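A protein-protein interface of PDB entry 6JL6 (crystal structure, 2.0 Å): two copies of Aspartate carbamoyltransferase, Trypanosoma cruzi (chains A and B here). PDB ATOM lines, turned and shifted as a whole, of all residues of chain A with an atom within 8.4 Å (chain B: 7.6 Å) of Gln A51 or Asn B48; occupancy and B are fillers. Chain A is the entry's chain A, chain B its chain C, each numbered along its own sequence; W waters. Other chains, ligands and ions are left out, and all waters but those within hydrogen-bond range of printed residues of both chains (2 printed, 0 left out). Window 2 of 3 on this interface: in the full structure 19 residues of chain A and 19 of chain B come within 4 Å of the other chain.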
ATOM      1  N   LEU A  47      15.448 -30.978 -19.587  1.00  0.00           N
ATOM      2  CA  LEU A  47      15.628 -29.548 -19.370  1.00  0.00           C
ATOM      3  C   LEU A  47      14.508 -28.995 -18.502  1.00  0.00           C
ATOM      4  O   LEU A  47      13.344 -29.380 -18.652  1.00  0.00           O
ATOM      5  CB  LEU A  47      15.682 -28.811 -20.712  1.00  0.00           C
ATOM      6  CG  LEU A  47      16.679 -29.353 -21.724  1.00  0.00           C
ATOM      7  CD1 LEU A  47      16.667 -28.522 -22.988  1.00  0.00           C
ATOM      8  CD2 LEU A  47      18.077 -29.390 -21.119  1.00  0.00           C
ATOM      9  N   ASN A  48      14.873 -28.099 -17.589  1.00  0.00           N
ATOM     10  CA  ASN A  48      13.924 -27.439 -16.696  1.00  0.00           C
ATOM     11  C   ASN A  48      13.944 -25.918 -16.820  1.00  0.00           C
ATOM     12  O   ASN A  48      13.588 -25.181 -15.872  1.00  0.00           O
ATOM     13  CB  ASN A  48      14.190 -27.867 -15.253  1.00  0.00           C
ATOM     14  CG  ASN A  48      13.005 -28.564 -14.644  1.00  0.00           C
ATOM     15  OD1 ASN A  48      11.882 -28.046 -14.681  1.00  0.00           O
ATOM     16  ND2 ASN A  48      13.233 -29.751 -14.092  1.00  0.00           N
ATOM     17  N   LEU A  49      14.259 -25.453 -18.020  1.00  0.00           N
ATOM     18  CA  LEU A  49      14.510 -24.050 -18.240  1.00  0.00           C
ATOM     19  C   LEU A  49      13.271 -23.174 -18.068  1.00  0.00           C
ATOM     20  O   LEU A  49      13.384 -22.072 -17.556  1.00  0.00           O
ATOM     21  CB  LEU A  49      15.151 -23.842 -19.606  1.00  0.00           C
ATOM     22  CG  LEU A  49      16.515 -24.519 -19.774  1.00  0.00           C
ATOM     23  CD1 LEU A  49      16.978 -24.374 -21.201  1.00  0.00           C
ATOM     24  CD2 LEU A  49      17.537 -23.915 -18.830  1.00  0.00           C
ATOM     25  N   LEU A  50      12.101 -23.667 -18.464  1.00  0.00           N
ATOM     26  CA  LEU A  50      10.875 -22.851 -18.474  1.00  0.00           C
ATOM     27  C   LEU A  50       9.772 -23.422 -17.567  1.00  0.00           C
ATOM     28  O   LEU A  50       8.586 -23.236 -17.819  1.00  0.00           O
ATOM     29  CB  LEU A  50      10.381 -22.672 -19.918  1.00  0.00           C
ATOM     30  CG  LEU A  50      11.211 -21.777 -20.866  1.00  0.00           C
ATOM     31  CD1 LEU A  50      10.500 -21.663 -22.206  1.00  0.00           C
ATOM     32  CD2 LEU A  50      11.490 -20.376 -20.313  1.00  0.00           C
ATOM     33  N   GLN A  51      10.186 -24.077 -16.481  1.00  0.00           N
ATOM     34  CA  GLN A  51       9.269 -24.565 -15.460  1.00  0.00           C
ATOM     35  C   GLN A  51       8.373 -23.431 -14.975  1.00  0.00           C
ATOM     36  O   GLN A  51       8.860 -22.350 -14.639  1.00  0.00           O
ATOM     37  CB  GLN A  51      10.033 -25.148 -14.277  1.00  0.00           C
ATOM     38  CG  GLN A  51       9.235 -26.178 -13.513  1.00  0.00           C
ATOM     39  CD  GLN A  51       9.903 -26.604 -12.218  1.00  0.00           C
ATOM     40  OE1 GLN A  51      11.057 -26.254 -11.944  1.00  0.00           O
ATOM     41  NE2 GLN A  51       9.172 -27.355 -11.407  1.00  0.00           N
ATOM     42  N   GLY A  52       7.064 -23.674 -14.986  1.00  0.00           N
ATOM     43  CA  GLY A  52       6.092 -22.696 -14.535  1.00  0.00           C
ATOM     44  C   GLY A  52       5.657 -21.655 -15.547  1.00  0.00           C
ATOM     45  O   GLY A  52       4.830 -20.801 -15.212  1.00  0.00           O
ATOM     46  N   ARG A  53       6.207 -21.699 -16.759  1.00  0.00           N
ATOM     47  CA  ARG A  53       5.850 -20.771 -17.822  1.00  0.00           C
ATOM     48  C   ARG A  53       4.854 -21.436 -18.772  1.00  0.00           C
ATOM     49  O   ARG A  53       4.865 -22.660 -18.969  1.00  0.00           O
ATOM     50  CB  ARG A  53       7.092 -20.294 -18.592  1.00  0.00           C
ATOM     51  CG  ARG A  53       8.254 -19.819 -17.723  1.00  0.00           C
ATOM     52  CD  ARG A  53       7.974 -18.565 -16.878  1.00  0.00           C
ATOM     53  NE  ARG A  53       9.013 -18.458 -15.832  1.00  0.00           N
ATOM     54  CZ  ARG A  53       8.829 -18.272 -14.512  1.00  0.00           C
ATOM     55  NH1 ARG A  53       7.621 -18.103 -13.976  1.00  0.00           N
ATOM     56  NH2 ARG A  53       9.891 -18.216 -13.704  1.00  0.00           N
ATOM     57  N   ILE A  54       3.971 -20.616 -19.329  1.00  0.00           N
ATOM     58  CA  ILE A  54       2.834 -21.102 -20.117  1.00  0.00           C
ATOM     59  C   ILE A  54       2.854 -20.545 -21.540  1.00  0.00           C
ATOM     60  O   ILE A  54       2.907 -19.314 -21.751  1.00  0.00           O
ATOM     61  CB  ILE A  54       1.477 -20.772 -19.437  1.00  0.00           C
ATOM     62  CG1 ILE A  54       1.334 -21.585 -18.149  1.00  0.00           C
ATOM     63  CG2 ILE A  54       0.301 -21.074 -20.371  1.00  0.00           C
ATOM     64  CD1 ILE A  54       0.063 -21.303 -17.372  1.00  0.00           C
ATOM     65  N   MET A  74       7.963 -26.478 -26.224  1.00  0.00           N
ATOM     66  CA  MET A  74       7.729 -25.910 -24.906  1.00  0.00           C
ATOM     67  C   MET A  74       7.918 -26.949 -23.795  1.00  0.00           C
ATOM     68  O   MET A  74       8.589 -26.681 -22.800  1.00  0.00           O
ATOM     69  CB  MET A  74       6.328 -25.306 -24.842  1.00  0.00           C
ATOM     70  CG  MET A  74       6.066 -24.482 -23.603  1.00  0.00           C
ATOM     71  SD  MET A  74       7.157 -23.056 -23.481  1.00  0.00           S
ATOM     72  CE  MET A  74       6.369 -22.193 -22.114  1.00  0.00           C
ATOM     73  N   ILE A  75       7.328 -28.129 -23.979  1.00  0.00           N
ATOM     74  CA  ILE A  75       7.397 -29.214 -23.011  1.00  0.00           C
ATOM     75  C   ILE A  75       8.838 -29.679 -22.764  1.00  0.00           C
ATOM     76  O   ILE A  75       9.215 -29.914 -21.612  1.00  0.00           O
ATOM     77  CB  ILE A  75       6.505 -30.400 -23.446  1.00  0.00           C
ATOM     78  CG1 ILE A  75       5.034 -30.032 -23.221  1.00  0.00           C
ATOM     79  CG2 ILE A  75       6.849 -31.681 -22.675  1.00  0.00           C
ATOM     80  CD1 ILE A  75       4.088 -30.831 -24.075  1.00  0.00           C
ATOM     81  N   LEU A  77      11.503 -27.924 -22.949  1.00  0.00           N
ATOM     82  CA  LEU A  77      12.166 -26.912 -22.119  1.00  0.00           C
ATOM     83  C   LEU A  77      11.683 -26.885 -20.661  1.00  0.00           C
ATOM     84  O   LEU A  77      12.149 -26.047 -19.864  1.00  0.00           O
ATOM     85  CB  LEU A  77      11.968 -25.513 -22.732  1.00  0.00           C
ATOM     86  CG  LEU A  77      12.584 -25.268 -24.095  1.00  0.00           C
ATOM     87  CD1 LEU A  77      12.004 -24.008 -24.726  1.00  0.00           C
ATOM     88  CD2 LEU A  77      14.094 -25.164 -23.989  1.00  0.00           C
ATOM     89  N   GLY A  78      10.764 -27.794 -20.318  1.00  0.00           N
ATOM     90  CA  GLY A  78      10.172 -27.868 -18.989  1.00  0.00           C
ATOM     91  C   GLY A  78       8.955 -26.976 -18.828  1.00  0.00           C
ATOM     92  O   GLY A  78       8.409 -26.893 -17.755  1.00  0.00           O
ATOM     93  N   GLY A  79       8.533 -26.299 -19.893  1.00  0.00           N
ATOM     94  CA  GLY A  79       7.376 -25.427 -19.833  1.00  0.00           C
ATOM     95  C   GLY A  79       6.070 -26.171 -19.962  1.00  0.00           C
ATOM     96  O   GLY A  79       6.046 -27.389 -20.114  1.00  0.00           O
ATOM     97  N   SER A  80       4.980 -25.413 -19.947  1.00  0.00           N
ATOM     98  CA  SER A  80       3.625 -25.971 -19.987  1.00  0.00           C
ATOM     99  C   SER A  80       2.788 -25.302 -21.077  1.00  0.00           C
ATOM    100  O   SER A  80       3.066 -24.179 -21.514  1.00  0.00           O
ATOM    101  CB  SER A  80       2.940 -25.769 -18.634  1.00  0.00           C
ATOM    102  OG  SER A  80       3.686 -26.372 -17.575  1.00  0.00           O
ATOM    103  N   ASP A 109       2.400 -16.743 -20.714  1.00  0.00           N
ATOM    104  CA  ASP A 109       3.700 -16.093 -20.895  1.00  0.00           C
ATOM    105  C   ASP A 109       3.993 -15.852 -22.365  1.00  0.00           C
ATOM    106  O   ASP A 109       4.700 -14.915 -22.693  1.00  0.00           O
ATOM    107  CB  ASP A 109       4.808 -16.925 -20.253  1.00  0.00           C
ATOM    108  CG  ASP A 109       4.675 -16.981 -18.755  1.00  0.00           C
ATOM    109  OD1 ASP A 109       5.220 -16.089 -18.083  1.00  0.00           O
ATOM    110  OD2 ASP A 109       4.021 -17.919 -18.235  1.00  0.00           O
ATOM    111  N   TRP A 323      13.062 -20.414 -25.634  1.00  0.00           N
ATOM    112  CA  TRP A 323      14.015 -20.181 -24.551  1.00  0.00           C
ATOM    113  C   TRP A 323      14.539 -18.767 -24.641  1.00  0.00           C
ATOM    114  O   TRP A 323      14.580 -18.051 -23.634  1.00  0.00           O
ATOM    115  CB  TRP A 323      15.164 -21.211 -24.592  1.00  0.00           C
ATOM    116  CG  TRP A 323      16.300 -20.996 -23.577  1.00  0.00           C
ATOM    117  CD1 TRP A 323      17.653 -21.077 -23.830  1.00  0.00           C
ATOM    118  CD2 TRP A 323      16.177 -20.657 -22.174  1.00  0.00           C
ATOM    119  NE1 TRP A 323      18.367 -20.819 -22.675  1.00  0.00           N
ATOM    120  CE2 TRP A 323      17.494 -20.572 -21.645  1.00  0.00           C
ATOM    121  CE3 TRP A 323      15.089 -20.440 -21.312  1.00  0.00           C
ATOM    122  CZ2 TRP A 323      17.749 -20.262 -20.292  1.00  0.00           C
ATOM    123  CZ3 TRP A 323      15.344 -20.125 -19.961  1.00  0.00           C
ATOM    124  CH2 TRP A 323      16.671 -20.034 -19.472  1.00  0.00           C
ATOM    125  N   LEU B   5       1.718 -19.847   1.952  1.00  0.00           N
ATOM    126  CA  LEU B   5       0.470 -20.177   1.271  1.00  0.00           C
ATOM    127  C   LEU B   5      -0.369 -21.227   2.005  1.00  0.00           C
ATOM    128  O   LEU B   5      -0.571 -22.332   1.487  1.00  0.00           O
ATOM    129  CB  LEU B   5       0.806 -20.675  -0.136  1.00  0.00           C
ATOM    130  CG  LEU B   5       1.697 -19.767  -0.983  1.00  0.00           C
ATOM    131  CD1 LEU B   5       2.035 -20.460  -2.292  1.00  0.00           C
ATOM    132  CD2 LEU B   5       1.022 -18.419  -1.218  1.00  0.00           C
ATOM    133  N   GLY B  44       8.017 -14.271 -10.159  1.00  0.00           N
ATOM    134  CA  GLY B  44       8.603 -15.314 -10.982  1.00  0.00           C
ATOM    135  C   GLY B  44       8.837 -16.612 -10.253  1.00  0.00           C
ATOM    136  O   GLY B  44       9.515 -17.474 -10.784  1.00  0.00           O
ATOM    137  N   GLU B  45       8.281 -16.775  -9.048  1.00  0.00           N
ATOM    138  CA  GLU B  45       8.429 -18.042  -8.323  1.00  0.00           C
ATOM    139  C   GLU B  45       7.552 -19.135  -8.938  1.00  0.00           C
ATOM    140  O   GLU B  45       6.443 -18.871  -9.423  1.00  0.00           O
ATOM    141  CB  GLU B  45       8.096 -17.902  -6.847  1.00  0.00           C
ATOM    142  CG  GLU B  45       9.016 -16.945  -6.106  1.00  0.00           C
ATOM    143  CD  GLU B  45       8.711 -16.869  -4.617  1.00  0.00           C
ATOM    144  OE1 GLU B  45       8.158 -17.853  -4.064  1.00  0.00           O
ATOM    145  OE2 GLU B  45       9.035 -15.824  -3.999  1.00  0.00           O
ATOM    146  N   VAL B  46       8.083 -20.351  -8.913  1.00  0.00           N
ATOM    147  CA  VAL B  46       7.417 -21.539  -9.415  1.00  0.00           C
ATOM    148  C   VAL B  46       6.851 -22.220  -8.174  1.00  0.00           C
ATOM    149  O   VAL B  46       7.559 -22.408  -7.194  1.00  0.00           O
ATOM    150  CB  VAL B  46       8.411 -22.485 -10.147  1.00  0.00           C
ATOM    151  CG1 VAL B  46       7.717 -23.754 -10.633  1.00  0.00           C
ATOM    152  CG2 VAL B  46       9.060 -21.774 -11.326  1.00  0.00           C
ATOM    153  N   LEU B  47       5.574 -22.569  -8.210  1.00  0.00           N
ATOM    154  CA  LEU B  47       4.937 -23.276  -7.113  1.00  0.00           C
ATOM    155  C   LEU B  47       4.817 -24.747  -7.494  1.00  0.00           C
ATOM    156  O   LEU B  47       4.538 -25.062  -8.653  1.00  0.00           O
ATOM    157  CB  LEU B  47       3.564 -22.664  -6.847  1.00  0.00           C
ATOM    158  CG  LEU B  47       3.541 -21.135  -6.711  1.00  0.00           C
ATOM    159  CD1 LEU B  47       2.123 -20.672  -6.403  1.00  0.00           C
ATOM    160  CD2 LEU B  47       4.519 -20.661  -5.635  1.00  0.00           C
ATOM    161  N   ASN B  48       5.035 -25.647  -6.534  1.00  0.00           N
ATOM    162  CA  ASN B  48       4.886 -27.090  -6.786  1.00  0.00           C
ATOM    163  C   ASN B  48       3.903 -27.818  -5.885  1.00  0.00           C
ATOM    164  O   ASN B  48       4.004 -29.029  -5.666  1.00  0.00           O
ATOM    165  CB  ASN B  48       6.253 -27.777  -6.840  1.00  0.00           C
ATOM    166  CG  ASN B  48       6.568 -28.283  -8.230  1.00  0.00           C
ATOM    167  OD1 ASN B  48       6.138 -29.372  -8.633  1.00  0.00           O
ATOM    168  ND2 ASN B  48       7.291 -27.480  -8.985  1.00  0.00           N
ATOM    169  N   LEU B  49       2.893 -27.087  -5.458  1.00  0.00           N
ATOM    170  CA  LEU B  49       1.926 -27.561  -4.487  1.00  0.00           C
ATOM    171  C   LEU B  49       1.061 -28.740  -4.970  1.00  0.00           C
ATOM    172  O   LEU B  49       0.659 -29.551  -4.170  1.00  0.00           O
ATOM    173  CB  LEU B  49       1.022 -26.401  -4.059  1.00  0.00           C
ATOM    174  CG  LEU B  49       1.750 -25.229  -3.380  1.00  0.00           C
ATOM    175  CD1 LEU B  49       0.804 -24.063  -3.130  1.00  0.00           C
ATOM    176  CD2 LEU B  49       2.400 -25.673  -2.079  1.00  0.00           C
ATOM    177  N   LEU B  50       0.747 -28.827  -6.263  1.00  0.00           N
ATOM    178  CA  LEU B  50      -0.165 -29.881  -6.721  1.00  0.00           C
ATOM    179  C   LEU B  50       0.477 -30.798  -7.759  1.00  0.00           C
ATOM    180  O   LEU B  50      -0.204 -31.383  -8.608  1.00  0.00           O
ATOM    181  CB  LEU B  50      -1.487 -29.274  -7.203  1.00  0.00           C
ATOM    182  CG  LEU B  50      -2.354 -28.560  -6.161  1.00  0.00           C
ATOM    183  CD1 LEU B  50      -3.605 -28.011  -6.834  1.00  0.00           C
ATOM    184  CD2 LEU B  50      -2.759 -29.461  -5.015  1.00  0.00           C
ATOM    185  N   GLN B  51       1.782 -30.996  -7.631  1.00  0.00           N
ATOM    186  CA  GLN B  51       2.480 -31.923  -8.506  1.00  0.00           C
ATOM    187  C   GLN B  51       1.825 -33.295  -8.394  1.00  0.00           C
ATOM    188  O   GLN B  51       1.477 -33.747  -7.303  1.00  0.00           O
ATOM    189  CB  GLN B  51       3.968 -31.996  -8.180  1.00  0.00           C
ATOM    190  CG  GLN B  51       4.775 -32.634  -9.300  1.00  0.00           C
ATOM    191  CD  GLN B  51       6.238 -32.851  -8.946  1.00  0.00           C
ATOM    192  OE1 GLN B  51       6.666 -32.632  -7.803  1.00  0.00           O
ATOM    193  NE2 GLN B  51       7.012 -33.302  -9.925  1.00  0.00           N
ATOM    194  N   GLY B  52       1.605 -33.918  -9.541  1.00  0.00           N
ATOM    195  CA  GLY B  52       1.025 -35.246  -9.601  1.00  0.00           C
ATOM    196  C   GLY B  52      -0.489 -35.287  -9.500  1.00  0.00           C
ATOM    197  O   GLY B  52      -1.047 -36.367  -9.505  1.00  0.00           O
ATOM    198  N   ILE B  75      -1.913 -25.485 -13.589  1.00  0.00           N
ATOM    199  CA  ILE B  75      -0.516 -25.535 -14.033  1.00  0.00           C
ATOM    200  C   ILE B  75       0.391 -24.650 -13.191  1.00  0.00           C
ATOM    201  O   ILE B  75       1.524 -25.032 -12.904  1.00  0.00           O
ATOM    202  CB  ILE B  75      -0.398 -25.137 -15.519  1.00  0.00           C
ATOM    203  CG1 ILE B  75      -0.901 -26.289 -16.384  1.00  0.00           C
ATOM    204  CG2 ILE B  75       1.035 -24.789 -15.910  1.00  0.00           C
ATOM    205  CD1 ILE B  75      -1.407 -25.834 -17.733  1.00  0.00           C
ATOM    206  N   ARG B  76      -0.077 -23.462 -12.819  1.00  0.00           N
ATOM    207  CA  ARG B  76       0.759 -22.579 -12.002  1.00  0.00           C
ATOM    208  C   ARG B  76       0.868 -23.051 -10.535  1.00  0.00           C
ATOM    209  O   ARG B  76       1.686 -22.522  -9.785  1.00  0.00           O
ATOM    210  CB  ARG B  76       0.276 -21.124 -12.096  1.00  0.00           C
ATOM    211  CG  ARG B  76       0.450 -20.562 -13.488  1.00  0.00           C
ATOM    212  CD  ARG B  76       0.293 -19.068 -13.540  1.00  0.00           C
ATOM    213  NE  ARG B  76       0.480 -18.539 -14.900  1.00  0.00           N
ATOM    214  CZ  ARG B  76       1.647 -18.254 -15.464  1.00  0.00           C
ATOM    215  NH1 ARG B  76       2.796 -18.435 -14.825  1.00  0.00           N
ATOM    216  NH2 ARG B  76       1.679 -17.772 -16.693  1.00  0.00           N
ATOM    217  N   LEU B  77       0.045 -24.019 -10.130  1.00  0.00           N
ATOM    218  CA  LEU B  77       0.219 -24.716  -8.853  1.00  0.00           C
ATOM    219  C   LEU B  77       1.105 -25.978  -8.973  1.00  0.00           C
ATOM    220  O   LEU B  77       1.330 -26.670  -7.979  1.00  0.00           O
ATOM    221  CB  LEU B  77      -1.131 -25.089  -8.262  1.00  0.00           C
ATOM    222  CG  LEU B  77      -2.039 -23.927  -7.835  1.00  0.00           C
ATOM    223  CD1 LEU B  77      -3.410 -24.446  -7.440  1.00  0.00           C
ATOM    224  CD2 LEU B  77      -1.426 -23.115  -6.696  1.00  0.00           C
ATOM    225  N   GLY B  78       1.602 -26.249 -10.183  1.00  0.00           N
ATOM    226  CA  GLY B  78       2.381 -27.439 -10.472  1.00  0.00           C
ATOM    227  C   GLY B  78       1.527 -28.648 -10.801  1.00  0.00           C
ATOM    228  O   GLY B  78       2.066 -29.733 -10.988  1.00  0.00           O
ATOM    229  N   GLY B  79       0.214 -28.461 -10.903  1.00  0.00           N
ATOM    230  CA  GLY B  79      -0.699 -29.561 -11.242  1.00  0.00           C
ATOM    231  C   GLY B  79      -0.687 -29.874 -12.736  1.00  0.00           C
ATOM    232  O   GLY B  79      -0.002 -29.212 -13.524  1.00  0.00           O
ATOM    233  N   TRP B 323      -5.876 -25.120  -4.695  1.00  0.00           N
ATOM    234  CA  TRP B 323      -4.978 -25.476  -3.602  1.00  0.00           C
ATOM    235  C   TRP B 323      -5.749 -25.759  -2.321  1.00  0.00           C
ATOM    236  O   TRP B 323      -5.477 -26.757  -1.647  1.00  0.00           O
ATOM    237  CB  TRP B 323      -3.922 -24.391  -3.393  1.00  0.00           C
ATOM    238  CG  TRP B 323      -3.020 -24.557  -2.197  1.00  0.00           C
ATOM    239  CD1 TRP B 323      -2.724 -23.596  -1.260  1.00  0.00           C
ATOM    240  CD2 TRP B 323      -2.294 -25.741  -1.801  1.00  0.00           C
ATOM    241  NE1 TRP B 323      -1.851 -24.102  -0.324  1.00  0.00           N
ATOM    242  CE2 TRP B 323      -1.573 -25.412  -0.624  1.00  0.00           C
ATOM    243  CE3 TRP B 323      -2.178 -27.041  -2.332  1.00  0.00           C
ATOM    244  CZ2 TRP B 323      -0.744 -26.334   0.039  1.00  0.00           C
ATOM    245  CZ3 TRP B 323      -1.349 -27.974  -1.669  1.00  0.00           C
ATOM    246  CH2 TRP B 323      -0.646 -27.609  -0.490  1.00  0.00           C
HETATM  247  O   HOH W   1       4.949 -16.678 -15.545  1.00  0.00           O
HETATM  248  O   HOH W   2       4.183 -19.845 -12.646  1.00  0.00           O
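NH1 of Arg B76 is in hydrogen-bond range of O of Gly A52, at 3.1 Å. The side-chain amide nitrogen (ND2) of Asn B48 sits close to the side-chain amide nitrogen (NE2) of Gln A51. The guanidinium group (NH2) of Arg A53 lies within hydrogen-bond range of the backbone carbonyl oxygen (O) of Gly B44 (3.0 Å). The guanidinium group (NH2) of Arg B76 is in salt-bridge range of the side-chain carboxylate (OD2) of Asp A109 (2.8 Å).
The side-chain amide oxygen (OD1) of Asn A48 sits close to the side-chain amide oxygen (OE1) of Gln A51 (3.4 Å). The backbone carbonyl oxygen (O) of Arg A53 lies within hydrogen-bond range of the backbone NH (N) of Ser A80 (2.9 Å). The side-chain amide oxygen (OD1) of Asn B48 sits close to the side-chain amide oxygen (OE1) of Gln B51 (3.4 Å). The backbone carbonyl oxygen (O) of Ile A54 sits at hydrogen-bond distance from the backbone NH (N) of Asp A109 (2.8 Å).
Among the printed residues, merely in contact across the chains: Gln A51 with Val B46, Ile A54 with Ile B75, Ile A54 with Arg B76 and Ser A80 with Ile B75.
Of chain B, only Val B46 (3.4 Å) and Asn B48 (3.1 Å) come within 4 Å of Gln A51. Met A74 touches none of the printed residues of chain B. Of the printed residues of chain B, Ser A80 touches Ile B75. Printed residues of chain A within 4 Å of Val B46: Gln A51 (3.4 Å). Leu B50 touches none of the printed residues of chain A.
Of the 16 printed residues of chain A, 6 touch a printed residue of chain B. Hydrophobic or aromatic side chains of chain A that line the printed part of chain B: Ile A54. Of the 16 printed residues of chain B, 5 touch a printed residue of chain A. Hydrophobic or aromatic side chains of chain B that line the printed part of chain A: Val B46 and Ile B75. Among the printed residues, 8 pairs touch across the chains.
Gln A51 touches Asn B48, but with the chains exchanged Asn A48 does not touch Gln B51 (8.3 Å). Of the 8 pairs that touch across the chains among the printed residues, none has its exchanged pair printed and touching as well.
Water W1 lies within hydrogen-bond range of the side-chain carboxylate of Asp A109 (2.6 Å), the guanidinium group of Arg B76 (2.9 Å) and the guanidinium group of Arg A53 (3.4 Å). Water W2 lies within hydrogen-bond range of O of Gly A52 (2.8 Å) and NH1 of Arg B76 (2.9 Å).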
